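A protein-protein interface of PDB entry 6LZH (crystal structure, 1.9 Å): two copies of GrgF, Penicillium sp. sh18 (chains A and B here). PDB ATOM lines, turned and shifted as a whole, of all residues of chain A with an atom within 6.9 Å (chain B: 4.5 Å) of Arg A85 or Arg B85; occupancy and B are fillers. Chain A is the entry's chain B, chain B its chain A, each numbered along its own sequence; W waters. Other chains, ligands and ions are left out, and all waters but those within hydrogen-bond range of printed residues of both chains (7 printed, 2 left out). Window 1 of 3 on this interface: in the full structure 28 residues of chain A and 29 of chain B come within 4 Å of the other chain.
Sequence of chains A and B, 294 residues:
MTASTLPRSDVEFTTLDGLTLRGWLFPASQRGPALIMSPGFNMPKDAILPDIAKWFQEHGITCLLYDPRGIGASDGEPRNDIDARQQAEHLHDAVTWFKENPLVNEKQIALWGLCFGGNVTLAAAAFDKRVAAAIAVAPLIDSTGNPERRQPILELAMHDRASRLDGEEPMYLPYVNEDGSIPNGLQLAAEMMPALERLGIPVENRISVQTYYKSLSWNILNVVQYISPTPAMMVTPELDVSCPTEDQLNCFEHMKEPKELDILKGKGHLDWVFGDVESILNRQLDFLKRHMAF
Water W6 lies within hydrogen-bond range of the side-chain hydroxyl (OG) of Ser B217 (2.8 Å), the guanidinium group (NH1) of Arg A85 (2.9 Å) and the backbone carbonyl oxygen (O) of Lys B214 (2.9 Å).
Water W1 bridges the backbone carbonyl oxygen (O) of Ser A217 (2.8 Å) and the backbone carbonyl oxygen (O) of Ser B217 (2.9 Å).
Water W5 lies within hydrogen-bond range of the guanidinium group of Arg B85 (2.8 Å), the side-chain hydroxyl of Ser A217 (2.9 Å) and the backbone carbonyl oxygen of Lys A214 (3.2 Å).
Water W3 lies within hydrogen-bond range of OH of Tyr A213 and O of Arg B85.
Water W4 bridges NZ of Lys A214 (2.9 Å) and OE1 of Glu B89 (3.3 Å).
Water W2 lies within hydrogen-bond range of the side-chain amino group of Lys B214 (2.9 Å) and the side-chain carboxylate of Glu A89 (3.3 Å).
Printed residues of chain B within 4 Å of Arg A85: Asp B83 (2.8 Å), Arg B85 (3.5 Å), Lys B214 (3.7 Å) and Ser B217 (3.6 Å).
Printed residues of chain A within 4 Å of Arg B85: Asp A83 (2.7 Å), Arg A85 (3.5 Å) and Ser A217 (3.6 Å).
Of the printed residues of chain B, Trp A218 touches Ser B217.
Of the printed residues of chain B, Asp A83 touches Arg B85 (2.7 Å).
Of the printed residues of chain A, Glu B89 touches Tyr A213 (3.5 Å).
Of the printed residues of chain A, Ser B217 touches Arg A85, Ser A217 and Trp A218.
The nearest printed residue of chain B that does not touch Arg A85 is Gln B86 (5.2 Å).
The nearest residue of chain A that does not touch Arg B85 is Lys A214 (4.1 Å).
Asp A83 touches Arg B85, and with the chains exchanged Arg A85 touches Asp B83.
Arg A85 touches Ser B217, and with the chains exchanged Ser A217 touches Arg B85.
Ser B217 touches its own counterpart, Ser A217.
Ser A217 touches Trp B218, and with the chains exchanged Trp A218 touches Ser B217.
Of the 10 pairs that touch across the chains among the printed residues, 8 have their exchanged pair printed and touching as well.
NH2 of Arg B85 touches NH2 of Arg A85 (3.5 Å).
Arg A85 touches Lys B214 (NH1 to CD, 3.7 Å).
Ser B217 touches Arg A85.
Tyr A213 touches Glu B89.
Arg B85 touches Ser A217.
Ser A217 touches Trp B218.
CZ3 of Trp A218 touches CB of Ser B217, at 3.7 Å.
N of Gln A86 sits at hydrogen-bond distance from OD1 of Asp A83 (3.2 Å).
NE of Arg B85 lies within salt-bridge range of OE2 of Glu B89.
The backbone carbonyl oxygen (O) of Lys A214 sits at hydrogen-bond distance from the side-chain hydroxyl (OG) of Ser A217 (3.1 Å).
The backbone NH (N) of Arg A85 is in hydrogen-bond range of the side-chain carboxylate (OD1) of Asp A83 (3.2 Å).
The backbone NH (N) of Asp A83 lies close to the side-chain amide nitrogen (NE2) of Gln A87, at 3.3 Å.
OE2 of Glu A89 lies within salt-bridge range of NE of Arg A85, 3.7 Å away.
Hydrophobic or aromatic side chains of chain A that line the printed part of chain B: Tyr A213 and Trp A218.
Along chain A the printed residues that touch a printed residue of chain B span positions 83 to 218.
Of the 10 printed residues of chain B, 6 touch a printed residue of chain A.
Hydrophobic or aromatic side chains of chain B within 4 Å of the printed part of chain A: Trp B218.
Among the printed residues, 10 pairs touch across the chains.
The guanidinium group (NH2) of Arg B85 is in salt-bridge range of the side-chain carboxylate (OD2) of Asp A83 (2.7 Å).
The backbone carbonyl oxygen of Ser A217 lies close to the backbone carbonyl oxygen of Ser B217, 3.4 Å away.
OD2 of Asp B83 is in salt-bridge range of NH2 of Arg A85 (2.8 Å).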
ATOM      1  N   ILE A  82      -0.959  11.201  32.440  1.00  0.00           N
ATOM      2  CA  ILE A  82      -0.603   9.788  32.433  1.00  0.00           C
ATOM      3  C   ILE A  82      -1.304   9.110  31.271  1.00  0.00           C
ATOM      4  O   ILE A  82      -2.518   9.270  31.087  1.00  0.00           O
ATOM      5  CB  ILE A  82      -0.970   9.117  33.765  1.00  0.00           C
ATOM      6  CG1 ILE A  82      -0.424   9.907  34.958  1.00  0.00           C
ATOM      7  CG2 ILE A  82      -0.424   7.718  33.806  1.00  0.00           C
ATOM      8  CD1 ILE A  82       1.003  10.341  34.817  1.00  0.00           C
ATOM      9  N   ASP A  83      -0.535   8.365  30.475  1.00  0.00           N
ATOM     10  CA  ASP A  83      -1.049   7.674  29.290  1.00  0.00           C
ATOM     11  C   ASP A  83      -0.441   6.276  29.313  1.00  0.00           C
ATOM     12  O   ASP A  83       0.716   6.108  28.923  1.00  0.00           O
ATOM     13  CB  ASP A  83      -0.680   8.442  28.022  1.00  0.00           C
ATOM     14  CG  ASP A  83      -1.217   7.790  26.745  1.00  0.00           C
ATOM     15  OD1 ASP A  83      -1.658   6.619  26.784  1.00  0.00           O
ATOM     16  OD2 ASP A  83      -1.184   8.458  25.689  1.00  0.00           O
ATOM     17  N   ALA A  84      -1.197   5.283  29.793  1.00  0.00           N
ATOM     18  CA  ALA A  84      -0.625   3.946  29.935  1.00  0.00           C
ATOM     19  C   ALA A  84      -0.183   3.374  28.588  1.00  0.00           C
ATOM     20  O   ALA A  84       0.901   2.787  28.475  1.00  0.00           O
ATOM     21  CB  ALA A  84      -1.626   3.015  30.614  1.00  0.00           C
ATOM     22  N   ARG A  85      -1.011   3.532  27.550  1.00  0.00           N
ATOM     23  CA  ARG A  85      -0.639   3.035  26.225  1.00  0.00           C
ATOM     24  C   ARG A  85       0.700   3.597  25.774  1.00  0.00           C
ATOM     25  O   ARG A  85       1.571   2.856  25.294  1.00  0.00           O
ATOM     26  CB  ARG A  85      -1.717   3.397  25.204  1.00  0.00           C
ATOM     27  CG  ARG A  85      -1.513   2.697  23.881  1.00  0.00           C
ATOM     28  CD  ARG A  85      -2.511   3.188  22.850  1.00  0.00           C
ATOM     29  NE  ARG A  85      -2.087   4.436  22.235  1.00  0.00           N
ATOM     30  CZ  ARG A  85      -2.742   5.021  21.235  1.00  0.00           C
ATOM     31  NH1 ARG A  85      -3.839   4.454  20.758  1.00  0.00           N
ATOM     32  NH2 ARG A  85      -2.307   6.165  20.713  1.00  0.00           N
ATOM     33  N   GLN A  86       0.881   4.910  25.908  1.00  0.00           N
ATOM     34  CA  GLN A  86       2.148   5.505  25.502  1.00  0.00           C
ATOM     35  C   GLN A  86       3.293   5.036  26.392  1.00  0.00           C
ATOM     36  O   GLN A  86       4.405   4.800  25.908  1.00  0.00           O
ATOM     37  CB  GLN A  86       2.044   7.033  25.534  1.00  0.00           C
ATOM     38  CG  GLN A  86       3.310   7.744  25.089  1.00  0.00           C
ATOM     39  CD  GLN A  86       3.255   9.245  25.327  1.00  0.00           C
ATOM     40  OE1 GLN A  86       2.758   9.705  26.354  1.00  0.00           O
ATOM     41  NE2 GLN A  86       3.788  10.014  24.386  1.00  0.00           N
ATOM     42  N   GLN A  87       3.057   4.929  27.705  1.00  0.00           N
ATOM     43  CA  GLN A  87       4.151   4.530  28.579  1.00  0.00           C
ATOM     44  C   GLN A  87       4.589   3.099  28.296  1.00  0.00           C
ATOM     45  O   GLN A  87       5.783   2.799  28.357  1.00  0.00           O
ATOM     46  CB  GLN A  87       3.751   4.748  30.033  1.00  0.00           C
ATOM     47  CG  GLN A  87       3.484   6.246  30.230  1.00  0.00           C
ATOM     48  CD  GLN A  87       3.138   6.666  31.637  1.00  0.00           C
ATOM     49  OE1 GLN A  87       3.478   5.984  32.619  1.00  0.00           O
ATOM     50  NE2 GLN A  87       2.439   7.812  31.744  1.00  0.00           N
ATOM     51  N   ALA A  88       3.645   2.216  27.948  1.00  0.00           N
ATOM     52  CA  ALA A  88       4.030   0.888  27.478  1.00  0.00           C
ATOM     53  C   ALA A  88       4.834   0.974  26.188  1.00  0.00           C
ATOM     54  O   ALA A  88       5.819   0.243  26.006  1.00  0.00           O
ATOM     55  CB  ALA A  88       2.794   0.014  27.266  1.00  0.00           C
ATOM     56  N   GLU A  89       4.422   1.850  25.266  1.00  0.00           N
ATOM     57  CA  GLU A  89       5.209   2.034  24.045  1.00  0.00           C
ATOM     58  C   GLU A  89       6.614   2.493  24.379  1.00  0.00           C
ATOM     59  O   GLU A  89       7.588   2.039  23.764  1.00  0.00           O
ATOM     60  CB  GLU A  89       4.536   3.049  23.108  1.00  0.00           C
ATOM     61  CG  GLU A  89       3.221   2.582  22.552  1.00  0.00           C
ATOM     62  CD  GLU A  89       2.675   3.565  21.519  1.00  0.00           C
ATOM     63  OE1 GLU A  89       3.351   3.801  20.499  1.00  0.00           O
ATOM     64  OE2 GLU A  89       1.592   4.115  21.748  1.00  0.00           O
ATOM     65  N   HIS A  90       6.747   3.406  25.350  1.00  0.00           N
ATOM     66  CA  HIS A  90       8.078   3.881  25.719  1.00  0.00           C
ATOM     67  C   HIS A  90       8.912   2.778  26.351  1.00  0.00           C
ATOM     68  O   HIS A  90      10.142   2.783  26.219  1.00  0.00           O
ATOM     69  CB  HIS A  90       7.970   5.101  26.647  1.00  0.00           C
ATOM     70  CG  HIS A  90       7.448   6.320  25.953  1.00  0.00           C
ATOM     71  ND1 HIS A  90       7.117   7.483  26.620  1.00  0.00           N
ATOM     72  CD2 HIS A  90       7.192   6.553  24.642  1.00  0.00           C
ATOM     73  CE1 HIS A  90       6.686   8.380  25.747  1.00  0.00           C
ATOM     74  NE2 HIS A  90       6.725   7.842  24.540  1.00  0.00           N
ATOM     75  N   HIS A  92       8.854  -0.220  25.190  1.00  0.00           N
ATOM     76  CA  HIS A  92       9.442  -0.848  24.010  1.00  0.00           C
ATOM     77  C   HIS A  92      10.695  -0.111  23.561  1.00  0.00           C
ATOM     78  O   HIS A  92      11.693  -0.735  23.178  1.00  0.00           O
ATOM     79  CB  HIS A  92       8.418  -0.884  22.867  1.00  0.00           C
ATOM     80  CG  HIS A  92       7.105  -1.490  23.251  1.00  0.00           C
ATOM     81  ND1 HIS A  92       6.985  -2.453  24.236  1.00  0.00           N
ATOM     82  CD2 HIS A  92       5.854  -1.269  22.783  1.00  0.00           C
ATOM     83  CE1 HIS A  92       5.714  -2.791  24.364  1.00  0.00           C
ATOM     84  NE2 HIS A  92       5.007  -2.092  23.489  1.00  0.00           N
ATOM     85  N   PHE A 116       1.039   1.720  39.354  1.00  0.00           N
ATOM     86  CA  PHE A 116       0.728   1.964  37.946  1.00  0.00           C
ATOM     87  C   PHE A 116       1.837   1.456  37.037  1.00  0.00           C
ATOM     88  O   PHE A 116       1.568   1.028  35.907  1.00  0.00           O
ATOM     89  CB  PHE A 116       0.500   3.452  37.700  1.00  0.00           C
ATOM     90  CG  PHE A 116       0.083   3.772  36.281  1.00  0.00           C
ATOM     91  CD1 PHE A 116      -1.231   3.610  35.881  1.00  0.00           C
ATOM     92  CD2 PHE A 116       1.011   4.241  35.361  1.00  0.00           C
ATOM     93  CE1 PHE A 116      -1.622   3.916  34.585  1.00  0.00           C
ATOM     94  CE2 PHE A 116       0.629   4.548  34.060  1.00  0.00           C
ATOM     95  CZ  PHE A 116      -0.685   4.385  33.672  1.00  0.00           C
ATOM     96  N   VAL A 120       1.611  -0.845  33.421  1.00  0.00           N
ATOM     97  CA  VAL A 120       2.334  -0.610  32.181  1.00  0.00           C
ATOM     98  C   VAL A 120       3.297  -1.748  31.887  1.00  0.00           C
ATOM     99  O   VAL A 120       3.506  -2.114  30.726  1.00  0.00           O
ATOM    100  CB  VAL A 120       3.063   0.740  32.263  1.00  0.00           C
ATOM    101  CG1 VAL A 120       3.893   0.947  31.026  1.00  0.00           C
ATOM    102  CG2 VAL A 120       2.042   1.855  32.416  1.00  0.00           C
ATOM    103  N   ALA A 123       1.311  -4.617  30.456  1.00  0.00           N
ATOM    104  CA  ALA A 123       0.932  -4.256  29.088  1.00  0.00           C
ATOM    105  C   ALA A 123       2.110  -4.389  28.137  1.00  0.00           C
ATOM    106  O   ALA A 123       1.975  -4.937  27.032  1.00  0.00           O
ATOM    107  CB  ALA A 123       0.388  -2.825  29.043  1.00  0.00           C
ATOM    108  N   PHE A 127       2.917  -7.161  24.621  1.00  0.00           N
ATOM    109  CA  PHE A 127       3.159  -6.815  23.228  1.00  0.00           C
ATOM    110  C   PHE A 127       4.567  -7.120  22.727  1.00  0.00           C
ATOM    111  O   PHE A 127       4.736  -7.326  21.519  1.00  0.00           O
ATOM    112  CB  PHE A 127       2.882  -5.322  23.016  1.00  0.00           C
ATOM    113  CG  PHE A 127       1.496  -4.914  23.384  1.00  0.00           C
ATOM    114  CD1 PHE A 127       0.416  -5.706  23.022  1.00  0.00           C
ATOM    115  CD2 PHE A 127       1.266  -3.734  24.076  1.00  0.00           C
ATOM    116  CE1 PHE A 127      -0.895  -5.328  23.366  1.00  0.00           C
ATOM    117  CE2 PHE A 127      -0.031  -3.349  24.416  1.00  0.00           C
ATOM    118  CZ  PHE A 127      -1.110  -4.148  24.054  1.00  0.00           C
ATOM    119  N   TYR A 213      -9.410  10.813  31.070  1.00  0.00           N
ATOM    120  CA  TYR A 213      -9.937  10.560  29.732  1.00  0.00           C
ATOM    121  C   TYR A 213      -9.249   9.358  29.084  1.00  0.00           C
ATOM    122  O   TYR A 213      -9.909   8.434  28.584  1.00  0.00           O
ATOM    123  CB  TYR A 213      -9.760  11.814  28.867  1.00  0.00           C
ATOM    124  CG  TYR A 213     -10.173  11.625  27.420  1.00  0.00           C
ATOM    125  CD1 TYR A 213      -9.279  11.141  26.478  1.00  0.00           C
ATOM    126  CD2 TYR A 213     -11.462  11.937  27.001  1.00  0.00           C
ATOM    127  CE1 TYR A 213      -9.656  10.955  25.164  1.00  0.00           C
ATOM    128  CE2 TYR A 213     -11.846  11.762  25.682  1.00  0.00           C
ATOM    129  CZ  TYR A 213     -10.951  11.270  24.778  1.00  0.00           C
ATOM    130  OH  TYR A 213     -11.331  11.097  23.482  1.00  0.00           O
ATOM    131  N   LYS A 214      -7.915   9.367  29.065  1.00  0.00           N
ATOM    132  CA  LYS A 214      -7.164   8.284  28.438  1.00  0.00           C
ATOM    133  C   LYS A 214      -7.413   6.953  29.135  1.00  0.00           C
ATOM    134  O   LYS A 214      -7.494   5.905  28.481  1.00  0.00           O
ATOM    135  CB  LYS A 214      -5.678   8.627  28.452  1.00  0.00           C
ATOM    136  CG  LYS A 214      -5.291   9.715  27.432  1.00  0.00           C
ATOM    137  CD  LYS A 214      -3.849  10.167  27.660  1.00  0.00           C
ATOM    138  CE  LYS A 214      -3.765  11.629  28.092  1.00  0.00           C
ATOM    139  NZ  LYS A 214      -3.625  12.528  26.902  1.00  0.00           N
ATOM    140  N   SER A 215      -7.560   6.975  30.456  1.00  0.00           N
ATOM    141  CA  SER A 215      -7.638   5.732  31.201  1.00  0.00           C
ATOM    142  C   SER A 215      -8.926   4.972  30.922  1.00  0.00           C
ATOM    143  O   SER A 215      -8.939   3.742  31.051  1.00  0.00           O
ATOM    144  CB  SER A 215      -7.483   6.012  32.700  1.00  0.00           C
ATOM    145  OG  SER A 215      -8.741   6.248  33.320  1.00  0.00           O
ATOM    146  N   SER A 217     -10.267   4.387  28.097  1.00  0.00           N
ATOM    147  CA  SER A 217     -10.028   3.522  26.955  1.00  0.00           C
ATOM    148  C   SER A 217      -8.868   2.555  27.191  1.00  0.00           C
ATOM    149  O   SER A 217      -8.437   1.878  26.248  1.00  0.00           O
ATOM    150  CB  SER A 217      -9.809   4.365  25.687  1.00  0.00           C
ATOM    151  OG  SER A 217      -8.546   5.014  25.656  1.00  0.00           O
ATOM    152  N   TRP A 218      -8.390   2.447  28.435  1.00  0.00           N
ATOM    153  CA  TRP A 218      -7.299   1.551  28.818  1.00  0.00           C
ATOM    154  C   TRP A 218      -7.798   0.532  29.833  1.00  0.00           C
ATOM    155  O   TRP A 218      -8.196   0.897  30.941  1.00  0.00           O
ATOM    156  CB  TRP A 218      -6.131   2.331  29.423  1.00  0.00           C
ATOM    157  CG  TRP A 218      -4.935   1.470  29.680  1.00  0.00           C
ATOM    158  CD1 TRP A 218      -4.499   1.000  30.890  1.00  0.00           C
ATOM    159  CD2 TRP A 218      -4.029   0.959  28.692  1.00  0.00           C
ATOM    160  NE1 TRP A 218      -3.348   0.251  30.716  1.00  0.00           N
ATOM    161  CE2 TRP A 218      -3.049   0.206  29.375  1.00  0.00           C
ATOM    162  CE3 TRP A 218      -3.935   1.087  27.295  1.00  0.00           C
ATOM    163  CZ2 TRP A 218      -1.996  -0.421  28.707  1.00  0.00           C
ATOM    164  CZ3 TRP A 218      -2.892   0.449  26.630  1.00  0.00           C
ATOM    165  CH2 TRP A 218      -1.932  -0.289  27.340  1.00  0.00           C
ATOM    166  N   ASP B  83      -5.474   5.022  14.252  1.00  0.00           N
ATOM    167  CA  ASP B  83      -5.444   5.120  15.711  1.00  0.00           C
ATOM    168  C   ASP B  83      -6.838   5.556  16.148  1.00  0.00           C
ATOM    169  O   ASP B  83      -7.163   6.743  16.074  1.00  0.00           O
ATOM    170  CB  ASP B  83      -4.372   6.109  16.169  1.00  0.00           C
ATOM    171  CG  ASP B  83      -4.189   6.120  17.680  1.00  0.00           C
ATOM    172  OD1 ASP B  83      -5.032   5.523  18.387  1.00  0.00           O
ATOM    173  OD2 ASP B  83      -3.205   6.727  18.151  1.00  0.00           O
ATOM    174  N   ALA B  84      -7.665   4.593  16.574  1.00  0.00           N
ATOM    175  CA  ALA B  84      -9.043   4.920  16.928  1.00  0.00           C
ATOM    176  C   ALA B  84      -9.094   5.928  18.064  1.00  0.00           C
ATOM    177  O   ALA B  84      -9.874   6.884  18.019  1.00  0.00           O
ATOM    178  CB  ALA B  84      -9.813   3.656  17.316  1.00  0.00           C
ATOM    179  N   ARG B  85      -8.281   5.719  19.111  1.00  0.00           N
ATOM    180  CA  ARG B  85      -8.288   6.657  20.227  1.00  0.00           C
ATOM    181  C   ARG B  85      -7.983   8.074  19.759  1.00  0.00           C
ATOM    182  O   ARG B  85      -8.688   9.024  20.120  1.00  0.00           O
ATOM    183  CB  ARG B  85      -7.279   6.229  21.292  1.00  0.00           C
ATOM    184  CG  ARG B  85      -7.342   7.120  22.500  1.00  0.00           C
ATOM    185  CD  ARG B  85      -6.252   6.727  23.505  1.00  0.00           C
ATOM    186  NE  ARG B  85      -5.011   7.432  23.210  1.00  0.00           N
ATOM    187  CZ  ARG B  85      -3.926   7.370  23.976  1.00  0.00           C
ATOM    188  NH1 ARG B  85      -3.938   6.626  25.070  1.00  0.00           N
ATOM    189  NH2 ARG B  85      -2.836   8.051  23.645  1.00  0.00           N
ATOM    190  N   GLN B  86      -6.931   8.237  18.958  1.00  0.00           N
ATOM    191  CA  GLN B  86      -6.581   9.574  18.481  1.00  0.00           C
ATOM    192  C   GLN B  86      -7.679  10.140  17.589  1.00  0.00           C
ATOM    193  O   GLN B  86      -7.954  11.345  17.610  1.00  0.00           O
ATOM    194  CB  GLN B  86      -5.265   9.539  17.705  1.00  0.00           C
ATOM    195  CG  GLN B  86      -4.855  10.917  17.178  1.00  0.00           C
ATOM    196  CD  GLN B  86      -3.677  10.879  16.209  1.00  0.00           C
ATOM    197  OE1 GLN B  86      -3.566   9.980  15.376  1.00  0.00           O
ATOM    198  NE2 GLN B  86      -2.806  11.873  16.301  1.00  0.00           N
ATOM    199  N   GLN B  87      -8.290   9.282  16.766  1.00  0.00           N
ATOM    200  CA  GLN B  87      -9.304   9.761  15.830  1.00  0.00           C
ATOM    201  C   GLN B  87     -10.546  10.212  16.579  1.00  0.00           C
ATOM    202  O   GLN B  87     -11.174  11.216  16.212  1.00  0.00           O
ATOM    203  CB  GLN B  87      -9.635   8.673  14.797  1.00  0.00           C
ATOM    204  CG  GLN B  87     -10.394   9.207  13.570  1.00  0.00           C
ATOM    205  CD  GLN B  87     -10.540   8.209  12.420  1.00  0.00           C
ATOM    206  OE1 GLN B  87      -9.659   7.351  12.174  1.00  0.00           O
ATOM    207  NE2 GLN B  87     -11.659   8.329  11.694  1.00  0.00           N
ATOM    208  N   ALA B  88     -10.905   9.497  17.649  1.00  0.00           N
ATOM    209  CA  ALA B  88     -11.993   9.961  18.500  1.00  0.00           C
ATOM    210  C   ALA B  88     -11.641  11.296  19.130  1.00  0.00           C
ATOM    211  O   ALA B  88     -12.488  12.192  19.214  1.00  0.00           O
ATOM    212  CB  ALA B  88     -12.291   8.930  19.595  1.00  0.00           C
ATOM    213  N   GLU B  89     -10.401  11.431  19.620  1.00  0.00           N
ATOM    214  CA  GLU B  89      -9.966  12.710  20.173  1.00  0.00           C
ATOM    215  C   GLU B  89     -10.125  13.819  19.147  1.00  0.00           C
ATOM    216  O   GLU B  89     -10.558  14.929  19.474  1.00  0.00           O
ATOM    217  CB  GLU B  89      -8.513  12.620  20.621  1.00  0.00           C
ATOM    218  CG  GLU B  89      -8.308  11.990  21.974  1.00  0.00           C
ATOM    219  CD  GLU B  89      -6.846  12.025  22.363  1.00  0.00           C
ATOM    220  OE1 GLU B  89      -6.319  13.113  22.687  1.00  0.00           O
ATOM    221  OE2 GLU B  89      -6.219  10.967  22.293  1.00  0.00           O
ATOM    222  N   LYS B 214      -1.957  -0.781  17.905  1.00  0.00           N
ATOM    223  CA  LYS B 214      -2.859   0.100  18.646  1.00  0.00           C
ATOM    224  C   LYS B 214      -4.263  -0.485  18.789  1.00  0.00           C
ATOM    225  O   LYS B 214      -4.931  -0.233  19.800  1.00  0.00           O
ATOM    226  CB  LYS B 214      -2.918   1.464  17.969  1.00  0.00           C
ATOM    227  CG  LYS B 214      -1.658   2.291  18.184  1.00  0.00           C
ATOM    228  CD  LYS B 214      -1.855   3.730  17.732  1.00  0.00           C
ATOM    229  CE  LYS B 214      -0.538   4.514  17.737  1.00  0.00           C
ATOM    230  NZ  LYS B 214       0.315   4.194  16.542  1.00  0.00           N
ATOM    231  N   SER B 217      -5.165  -2.616  21.961  1.00  0.00           N
ATOM    232  CA  SER B 217      -5.469  -1.907  23.200  1.00  0.00           C
ATOM    233  C   SER B 217      -6.761  -1.113  23.115  1.00  0.00           C
ATOM    234  O   SER B 217      -7.083  -0.370  24.054  1.00  0.00           O
ATOM    235  CB  SER B 217      -4.331  -0.962  23.585  1.00  0.00           C
ATOM    236  OG  SER B 217      -4.018  -0.073  22.510  1.00  0.00           O
ATOM    237  N   TRP B 218      -7.485  -1.231  22.010  1.00  0.00           N
ATOM    238  CA  TRP B 218      -8.711  -0.478  21.775  1.00  0.00           C
ATOM    239  C   TRP B 218      -9.860  -1.473  21.701  1.00  0.00           C
ATOM    240  O   TRP B 218      -9.883  -2.340  20.822  1.00  0.00           O
ATOM    241  CB  TRP B 218      -8.598   0.338  20.485  1.00  0.00           C
ATOM    242  CG  TRP B 218      -9.790   1.190  20.225  1.00  0.00           C
ATOM    243  CD1 TRP B 218     -10.811   0.920  19.361  1.00  0.00           C
ATOM    244  CD2 TRP B 218     -10.096   2.449  20.837  1.00  0.00           C
ATOM    245  NE1 TRP B 218     -11.744   1.941  19.396  1.00  0.00           N
ATOM    246  CE2 TRP B 218     -11.322   2.894  20.288  1.00  0.00           C
ATOM    247  CE3 TRP B 218      -9.449   3.252  21.785  1.00  0.00           C
ATOM    248  CZ2 TRP B 218     -11.913   4.103  20.658  1.00  0.00           C
ATOM    249  CZ3 TRP B 218     -10.045   4.457  22.160  1.00  0.00           C
ATOM    250  CH2 TRP B 218     -11.261   4.874  21.586  1.00  0.00           C
HETATM  251  O   HOH W   1      -6.438   2.433  24.371  1.00  0.00           O
HETATM  252  O   HOH W   2       2.090   2.345  17.864  1.00  0.00           O
HETATM  253  O   HOH W   3     -10.388   8.538  22.681  1.00  0.00           O
HETATM  254  O   HOH W   4      -6.307  13.043  26.014  1.00  0.00           O
HETATM  255  O   HOH W   5      -5.699   4.673  26.130  1.00  0.00           O
HETATM  256  O   HOH W   6      -5.419   2.113  21.506  1.00  0.00           O
HETATM  257  O   HOH W   7       2.172   5.989  18.903  1.00  0.00           O
